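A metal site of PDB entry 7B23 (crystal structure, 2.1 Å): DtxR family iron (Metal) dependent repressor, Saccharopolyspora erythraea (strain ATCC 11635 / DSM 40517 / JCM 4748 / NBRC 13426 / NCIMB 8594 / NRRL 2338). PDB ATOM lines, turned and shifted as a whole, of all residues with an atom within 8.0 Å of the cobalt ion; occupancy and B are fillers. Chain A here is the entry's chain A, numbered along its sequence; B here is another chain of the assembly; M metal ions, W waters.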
ATOM      1  N   ARG A  15      30.645  -5.198  28.092  1.00  0.00           N
ATOM      2  CA  ARG A  15      29.845  -5.747  26.963  1.00  0.00           C
ATOM      3  C   ARG A  15      29.162  -7.054  27.393  1.00  0.00           C
ATOM      4  O   ARG A  15      28.051  -7.311  26.900  1.00  0.00           O
ATOM      5  CB  ARG A  15      30.703  -5.968  25.711  1.00  0.00           C
ATOM      6  CG  ARG A  15      29.967  -5.699  24.413  1.00  0.00           C
ATOM      7  CD  ARG A  15      30.412  -6.634  23.302  1.00  0.00           C
ATOM      8  NE  ARG A  15      29.869  -7.971  23.483  1.00  0.00           N
ATOM      9  CZ  ARG A  15      30.388  -9.088  22.970  1.00  0.00           C
ATOM     10  NH1 ARG A  15      31.481  -9.038  22.234  1.00  0.00           N
ATOM     11  NH2 ARG A  15      29.802 -10.253  23.200  1.00  0.00           N
ATOM     12  N   ASP A  19      25.328  -7.748  27.203  1.00  0.00           N
ATOM     13  CA  ASP A  19      24.792  -9.008  26.616  1.00  0.00           C
ATOM     14  C   ASP A  19      23.700  -9.559  27.530  1.00  0.00           C
ATOM     15  O   ASP A  19      22.591  -9.819  27.023  1.00  0.00           O
ATOM     16  CB  ASP A  19      25.884 -10.062  26.422  1.00  0.00           C
ATOM     17  CG  ASP A  19      26.904  -9.708  25.366  1.00  0.00           C
ATOM     18  OD1 ASP A  19      26.666  -8.730  24.631  1.00  0.00           O
ATOM     19  OD2 ASP A  19      27.943 -10.405  25.282  1.00  0.00           O
ATOM     20  N   MET A  78      30.031  -2.238  21.759  1.00  0.00           N
ATOM     21  CA  MET A  78      28.997  -3.023  21.018  1.00  0.00           C
ATOM     22  C   MET A  78      28.807  -2.454  19.612  1.00  0.00           C
ATOM     23  O   MET A  78      28.674  -3.252  18.661  1.00  0.00           O
ATOM     24  CB  MET A  78      27.662  -3.005  21.761  1.00  0.00           C
ATOM     25  CG  MET A  78      26.633  -3.959  21.178  1.00  0.00           C
ATOM     26  SD  MET A  78      27.197  -5.679  21.184  1.00  0.00           S
ATOM     27  CE  MET A  78      26.773  -6.145  22.864  1.00  0.00           C
ATOM     28  N   HIS A  81      31.650  -3.501  17.514  1.00  0.00           N
ATOM     29  CA  HIS A  81      31.446  -4.958  17.328  1.00  0.00           C
ATOM     30  C   HIS A  81      30.532  -5.227  16.122  1.00  0.00           C
ATOM     31  O   HIS A  81      30.949  -5.966  15.208  1.00  0.00           O
ATOM     32  CB  HIS A  81      30.870  -5.576  18.600  1.00  0.00           C
ATOM     33  CG  HIS A  81      30.661  -7.046  18.518  1.00  0.00           C
ATOM     34  ND1 HIS A  81      31.659  -7.939  18.843  1.00  0.00           N
ATOM     35  CD2 HIS A  81      29.591  -7.779  18.162  1.00  0.00           C
ATOM     36  CE1 HIS A  81      31.202  -9.168  18.687  1.00  0.00           C
ATOM     37  NE2 HIS A  81      29.936  -9.093  18.270  1.00  0.00           N
ATOM     38  N   ARG A  82      29.342  -4.618  16.109  1.00  0.00           N
ATOM     39  CA  ARG A  82      28.265  -4.925  15.129  1.00  0.00           C
ATOM     40  C   ARG A  82      28.560  -4.240  13.789  1.00  0.00           C
ATOM     41  O   ARG A  82      28.072  -4.753  12.773  1.00  0.00           O
ATOM     42  CB  ARG A  82      26.911  -4.566  15.742  1.00  0.00           C
ATOM     43  CG  ARG A  82      26.535  -5.507  16.880  1.00  0.00           C
ATOM     44  CD  ARG A  82      25.262  -5.186  17.648  1.00  0.00           C
ATOM     45  NE  ARG A  82      25.059  -6.238  18.642  1.00  0.00           N
ATOM     46  CZ  ARG A  82      24.192  -6.192  19.648  1.00  0.00           C
ATOM     47  NH1 ARG A  82      23.391  -5.148  19.819  1.00  0.00           N
ATOM     48  NH2 ARG A  82      24.116  -7.218  20.490  1.00  0.00           N
ATOM     49  N   GLU A  85      31.279  -6.644  12.261  1.00  0.00           N
ATOM     50  CA  GLU A  85      30.561  -7.850  11.771  1.00  0.00           C
ATOM     51  C   GLU A  85      29.964  -7.573  10.383  1.00  0.00           C
ATOM     52  O   GLU A  85      30.098  -8.453   9.510  1.00  0.00           O
ATOM     53  CB  GLU A  85      29.464  -8.276  12.746  1.00  0.00           C
ATOM     54  CG  GLU A  85      29.995  -8.957  13.993  1.00  0.00           C
ATOM     55  CD  GLU A  85      28.930  -9.387  14.984  1.00  0.00           C
ATOM     56  OE1 GLU A  85      27.859  -8.745  15.019  1.00  0.00           O
ATOM     57  OE2 GLU A  85      29.164 -10.369  15.726  1.00  0.00           O
ATOM     58  N   VAL A  99      32.656 -14.874  12.057  1.00  0.00           N
ATOM     59  CA  VAL A  99      32.681 -13.384  11.991  1.00  0.00           C
ATOM     60  C   VAL A  99      32.655 -12.787  13.405  1.00  0.00           C
ATOM     61  O   VAL A  99      33.438 -11.843  13.647  1.00  0.00           O
ATOM     62  CB  VAL A  99      31.538 -12.822  11.108  1.00  0.00           C
ATOM     63  CG1 VAL A  99      31.211 -11.374  11.421  1.00  0.00           C
ATOM     64  CG2 VAL A  99      31.848 -12.999   9.631  1.00  0.00           C
ATOM     65  N   HIS A 100      31.819 -13.308  14.307  1.00  0.00           N
ATOM     66  CA  HIS A 100      31.696 -12.810  15.702  1.00  0.00           C
ATOM     67  C   HIS A 100      33.064 -12.880  16.396  1.00  0.00           C
ATOM     68  O   HIS A 100      33.475 -11.852  16.969  1.00  0.00           O
ATOM     69  CB  HIS A 100      30.647 -13.601  16.495  1.00  0.00           C
ATOM     70  CG  HIS A 100      30.617 -13.251  17.946  1.00  0.00           C
ATOM     71  ND1 HIS A 100      29.935 -12.155  18.428  1.00  0.00           N
ATOM     72  CD2 HIS A 100      31.202 -13.842  19.016  1.00  0.00           C
ATOM     73  CE1 HIS A 100      30.086 -12.089  19.728  1.00  0.00           C
ATOM     74  NE2 HIS A 100      30.857 -13.108  20.122  1.00  0.00           N
ATOM     75  N   LEU A 101      33.740 -14.026  16.329  1.00  0.00           N
ATOM     76  CA  LEU A 101      35.043 -14.286  17.002  1.00  0.00           C
ATOM     77  C   LEU A 101      36.059 -13.210  16.575  1.00  0.00           C
ATOM     78  O   LEU A 101      36.853 -12.788  17.434  1.00  0.00           O
ATOM     79  CB  LEU A 101      35.537 -15.694  16.643  1.00  0.00           C
ATOM     80  CG  LEU A 101      36.847 -16.126  17.310  1.00  0.00           C
ATOM     81  CD1 LEU A 101      36.688 -16.175  18.825  1.00  0.00           C
ATOM     82  CD2 LEU A 101      37.307 -17.475  16.771  1.00  0.00           C
ATOM     83  N   GLU A 102      36.023 -12.805  15.303  1.00  0.00           N
ATOM     84  CA  GLU A 102      36.882 -11.736  14.742  1.00  0.00           C
ATOM     85  C   GLU A 102      36.472 -10.388  15.348  1.00  0.00           C
ATOM     86  O   GLU A 102      37.345  -9.670  15.858  1.00  0.00           O
ATOM     87  CB  GLU A 102      36.754 -11.697  13.218  1.00  0.00           C
ATOM     88  CG  GLU A 102      37.912 -11.003  12.529  1.00  0.00           C
ATOM     89  CD  GLU A 102      39.221 -11.794  12.519  1.00  0.00           C
ATOM     90  OE1 GLU A 102      39.146 -13.037  12.517  1.00  0.00           O
ATOM     91  OE2 GLU A 102      40.295 -11.168  12.507  1.00  0.00           O
ATOM     92  N   ALA A 103      35.172 -10.065  15.290  1.00  0.00           N
ATOM     93  CA  ALA A 103      34.559  -8.831  15.833  1.00  0.00           C
ATOM     94  C   ALA A 103      34.754  -8.753  17.342  1.00  0.00           C
ATOM     95  O   ALA A 103      34.738  -7.663  17.922  1.00  0.00           O
ATOM     96  CB  ALA A 103      33.098  -8.785  15.451  1.00  0.00           C
ATOM     97  N   CSD A 104      34.935  -9.911  17.989  1.00  0.00           N
ATOM     98  CA  CSD A 104      35.205  -9.971  19.421  1.00  0.00           C
ATOM     99  CB  CSD A 104      35.202 -11.419  19.927  1.00  0.00           C
ATOM    100  SG  CSD A 104      34.243 -11.588  21.467  1.00  0.00           S
ATOM    101  C   CSD A 104      36.544  -9.296  19.741  1.00  0.00           C
ATOM    102  O   CSD A 104      36.747  -8.828  20.858  1.00  0.00           O
ATOM    103  OD1 CSD A 104      35.004 -10.832  22.501  1.00  0.00           O
ATOM    104  OD2 CSD A 104      32.837 -10.870  21.294  1.00  0.00           O
ATOM    105  N   GLU A 107      36.548  -5.083  17.990  1.00  0.00           N
ATOM    106  CA  GLU A 107      35.707  -4.120  18.755  1.00  0.00           C
ATOM    107  C   GLU A 107      36.558  -3.267  19.713  1.00  0.00           C
ATOM    108  O   GLU A 107      36.028  -2.241  20.187  1.00  0.00           O
ATOM    109  CB  GLU A 107      34.602  -4.842  19.523  1.00  0.00           C
ATOM    110  CG  GLU A 107      35.095  -5.777  20.620  1.00  0.00           C
ATOM    111  CD  GLU A 107      34.014  -6.611  21.283  1.00  0.00           C
ATOM    112  OE1 GLU A 107      32.823  -6.369  21.007  1.00  0.00           O
ATOM    113  OE2 GLU A 107      34.364  -7.490  22.094  1.00  0.00           O
ATOM    114  N   SER A 128      23.201  -5.683  13.093  1.00  0.00           N
ATOM    115  CA  SER A 128      24.299  -6.643  12.785  1.00  0.00           C
ATOM    116  C   SER A 128      23.784  -7.682  11.791  1.00  0.00           C
ATOM    117  O   SER A 128      22.580  -7.761  11.561  1.00  0.00           O
ATOM    118  CB  SER A 128      24.810  -7.293  14.061  1.00  0.00           C
ATOM    119  OG  SER A 128      23.870  -8.234  14.563  1.00  0.00           O
ATOM    120  N   PRO A 129      24.666  -8.505  11.172  1.00  0.00           N
ATOM    121  CA  PRO A 129      24.225  -9.598  10.308  1.00  0.00           C
ATOM    122  C   PRO A 129      23.360 -10.632  11.035  1.00  0.00           C
ATOM    123  O   PRO A 129      22.696 -11.400  10.369  1.00  0.00           O
ATOM    124  CB  PRO A 129      25.529 -10.250   9.834  1.00  0.00           C
ATOM    125  CG  PRO A 129      26.589  -9.188  10.034  1.00  0.00           C
ATOM    126  CD  PRO A 129      26.135  -8.418  11.258  1.00  0.00           C
ATOM    127  N   TYR A 130      23.391 -10.645  12.376  1.00  0.00           N
ATOM    128  CA  TYR A 130      22.651 -11.578  13.253  1.00  0.00           C
ATOM    129  C   TYR A 130      21.393 -10.894  13.809  1.00  0.00           C
ATOM    130  O   TYR A 130      20.752 -11.464  14.700  1.00  0.00           O
ATOM    131  CB  TYR A 130      23.598 -12.112  14.326  1.00  0.00           C
ATOM    132  CG  TYR A 130      24.916 -12.572  13.755  1.00  0.00           C
ATOM    133  CD1 TYR A 130      24.995 -13.725  13.002  1.00  0.00           C
ATOM    134  CD2 TYR A 130      26.070 -11.815  13.906  1.00  0.00           C
ATOM    135  CE1 TYR A 130      26.199 -14.145  12.448  1.00  0.00           C
ATOM    136  CE2 TYR A 130      27.276 -12.216  13.362  1.00  0.00           C
ATOM    137  CZ  TYR A 130      27.336 -13.388  12.627  1.00  0.00           C
ATOM    138  OH  TYR A 130      28.512 -13.794  12.076  1.00  0.00           O
ATOM    139  N   ASN A 132      20.805  -8.107  15.494  1.00  0.00           N
ATOM    140  CA  ASN A 132      20.886  -7.312  16.754  1.00  0.00           C
ATOM    141  C   ASN A 132      21.034  -5.835  16.400  1.00  0.00           C
ATOM    142  O   ASN A 132      21.914  -5.472  15.633  1.00  0.00           O
ATOM    143  CB  ASN A 132      22.046  -7.768  17.637  1.00  0.00           C
ATOM    144  CG  ASN A 132      21.981  -9.241  17.980  1.00  0.00           C
ATOM    145  OD1 ASN A 132      20.928  -9.745  18.358  1.00  0.00           O
ATOM    146  ND2 ASN A 132      23.092  -9.943  17.836  1.00  0.00           N
ATOM    147  N   ILE B 172      19.699 -13.091  16.839  1.00  0.00           N
ATOM    148  CA  ILE B 172      20.560 -14.127  17.493  1.00  0.00           C
ATOM    149  C   ILE B 172      21.564 -13.392  18.380  1.00  0.00           C
ATOM    150  O   ILE B 172      22.418 -12.676  17.827  1.00  0.00           O
ATOM    151  CB  ILE B 172      21.259 -15.001  16.436  1.00  0.00           C
ATOM    152  CG1 ILE B 172      20.251 -15.742  15.543  1.00  0.00           C
ATOM    153  CG2 ILE B 172      22.247 -15.955  17.092  1.00  0.00           C
ATOM    154  CD1 ILE B 172      20.876 -16.418  14.341  1.00  0.00           C
ATOM    155  N   ALA B 173      21.466 -13.543  19.702  1.00  0.00           N
ATOM    156  CA  ALA B 173      22.301 -12.836  20.691  1.00  0.00           C
ATOM    157  C   ALA B 173      23.765 -13.248  20.535  1.00  0.00           C
ATOM    158  O   ALA B 173      24.015 -14.295  19.910  1.00  0.00           O
ATOM    159  CB  ALA B 173      21.810 -13.095  22.094  1.00  0.00           C
ATOM    160  N   GLU B 174      24.673 -12.455  21.103  1.00  0.00           N
ATOM    161  CA  GLU B 174      26.147 -12.607  21.008  1.00  0.00           C
ATOM    162  C   GLU B 174      26.586 -13.925  21.662  1.00  0.00           C
ATOM    163  O   GLU B 174      27.577 -14.515  21.201  1.00  0.00           O
ATOM    164  CB  GLU B 174      26.863 -11.440  21.679  1.00  0.00           C
ATOM    165  CG  GLU B 174      26.436 -10.067  21.173  1.00  0.00           C
ATOM    166  CD  GLU B 174      26.661  -9.807  19.702  1.00  0.00           C
ATOM    167  OE1 GLU B 174      25.988  -8.914  19.150  1.00  0.00           O
ATOM    168  OE2 GLU B 174      27.523 -10.482  19.109  1.00  0.00           O
ATOM    169  N   HIS B 175      25.866 -14.359  22.703  1.00  0.00           N
ATOM    170  CA  HIS B 175      26.134 -15.600  23.486  1.00  0.00           C
ATOM    171  C   HIS B 175      26.057 -16.832  22.563  1.00  0.00           C
ATOM    172  O   HIS B 175      26.918 -17.705  22.692  1.00  0.00           O
ATOM    173  CB  HIS B 175      25.183 -15.663  24.679  1.00  0.00           C
ATOM    174  CG  HIS B 175      25.153 -16.979  25.388  1.00  0.00           C
ATOM    175  ND1 HIS B 175      26.299 -17.560  25.921  1.00  0.00           N
ATOM    176  CD2 HIS B 175      24.130 -17.817  25.678  1.00  0.00           C
ATOM    177  CE1 HIS B 175      25.981 -18.707  26.482  1.00  0.00           C
ATOM    178  NE2 HIS B 175      24.645 -18.882  26.354  1.00  0.00           N
ATOM    179  N   VAL B 176      25.063 -16.863  21.659  1.00  0.00           N
ATOM    180  CA  VAL B 176      24.856 -17.965  20.675  1.00  0.00           C
ATOM    181  C   VAL B 176      25.996 -17.959  19.653  1.00  0.00           C
ATOM    182  O   VAL B 176      26.492 -19.062  19.310  1.00  0.00           O
ATOM    183  CB  VAL B 176      23.479 -17.842  19.977  1.00  0.00           C
ATOM    184  CG1 VAL B 176      23.295 -18.888  18.895  1.00  0.00           C
ATOM    185  CG2 VAL B 176      22.333 -17.894  20.972  1.00  0.00           C
ATOM    186  N   GLN B 177      26.413 -16.770  19.209  1.00  0.00           N
ATOM    187  CA  GLN B 177      27.419 -16.557  18.124  1.00  0.00           C
ATOM    188  C   GLN B 177      28.785 -17.115  18.544  1.00  0.00           C
ATOM    189  O   GLN B 177      29.594 -17.407  17.645  1.00  0.00           O
ATOM    190  CB  GLN B 177      27.550 -15.079  17.797  1.00  0.00           C
ATOM    191  CG  GLN B 177      26.253 -14.432  17.310  1.00  0.00           C
ATOM    192  CD  GLN B 177      26.403 -12.946  17.112  1.00  0.00           C
ATOM    193  OE1 GLN B 177      27.466 -12.457  16.745  1.00  0.00           O
ATOM    194  NE2 GLN B 177      25.323 -12.220  17.325  1.00  0.00           N
ATOM    195  N   LEU B 178      29.033 -17.234  19.858  1.00  0.00           N
ATOM    196  CA  LEU B 178      30.337 -17.609  20.462  1.00  0.00           C
ATOM    197  C   LEU B 178      30.705 -19.062  20.108  1.00  0.00           C
ATOM    198  O   LEU B 178      31.914 -19.364  20.121  1.00  0.00           O
ATOM    199  CB  LEU B 178      30.243 -17.407  21.977  1.00  0.00           C
ATOM    200  CG  LEU B 178      31.564 -17.130  22.705  1.00  0.00           C
ATOM    201  CD1 LEU B 178      32.275 -15.910  22.121  1.00  0.00           C
ATOM    202  CD2 LEU B 178      31.320 -16.931  24.194  1.00  0.00           C
ATOM    203  N   MET B 183      26.463 -22.308  15.218  1.00  0.00           N
ATOM    204  CA  MET B 183      26.097 -21.268  14.213  1.00  0.00           C
ATOM    205  C   MET B 183      26.067 -21.900  12.811  1.00  0.00           C
ATOM    206  O   MET B 183      25.118 -21.599  12.063  1.00  0.00           O
ATOM    207  CB  MET B 183      27.089 -20.090  14.241  1.00  0.00           C
ATOM    208  CG  MET B 183      26.915 -19.190  15.455  1.00  0.00           C
ATOM    209  SD  MET B 183      25.360 -18.257  15.455  1.00  0.00           S
ATOM    210  CE  MET B 183      25.722 -16.987  14.248  1.00  0.00           C
HETATM  211 CO    CO M   1      28.704 -10.781  17.538  1.00  0.00          CO
HETATM  212  O   HOH W   1      26.147  -9.584  16.651  1.00  0.00           O
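Of the 25 residues printed, 5 come within 4 Å of the cobalt ion.
OD2 of CSD 104 lies within hydrogen-bond range of a ring nitrogen (NE2) of His 100 (3.2 Å). The side-chain amide nitrogen of Gln 177 of chain B sits at hydrogen-bond distance from the backbone carbonyl oxygen of Ile 172 of chain B. The side-chain amide nitrogen (NE2) of Gln 177 of chain B lies close to the side-chain amide nitrogen (ND2) of Asn 132. ND1 of His 81 lies within hydrogen-bond range of OE1 of Glu 107 (2.9 Å). NH2 of Arg 82 is in salt-bridge range of OE1 of Glu 174 of chain B, 2.9 Å away. ND1 of His 81 sits at hydrogen-bond distance from O of Ala 103 (3.2 Å). The side-chain carboxylate (OE1) of Glu 174 of chain B lies within hydrogen-bond range of the side-chain amide nitrogen (ND2) of Asn 132 (3.3 Å).
The cobalt ion is bound by OE2 of Glu 85 (1.9 Å), OE2 of Glu 174 of chain B (2.0 Å), ND1 of His 100 (2.0 Å), NE2 of His 81 (2.2 Å) and OE1 of Gln 177 of chain B (2.2 Å). The cobalt ion has five donor atoms within binding distance.
Water W1 lies within hydrogen-bond range of the side-chain carboxylate (OE1) of Glu 85, the side-chain carboxylate (OE1) of Glu 174 of chain B, the side-chain amide nitrogen (NE2) of Gln 177 of chain B, the side-chain amide nitrogen (ND2) of Asn 132 and the side-chain hydroxyl (OG) of Ser 128.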
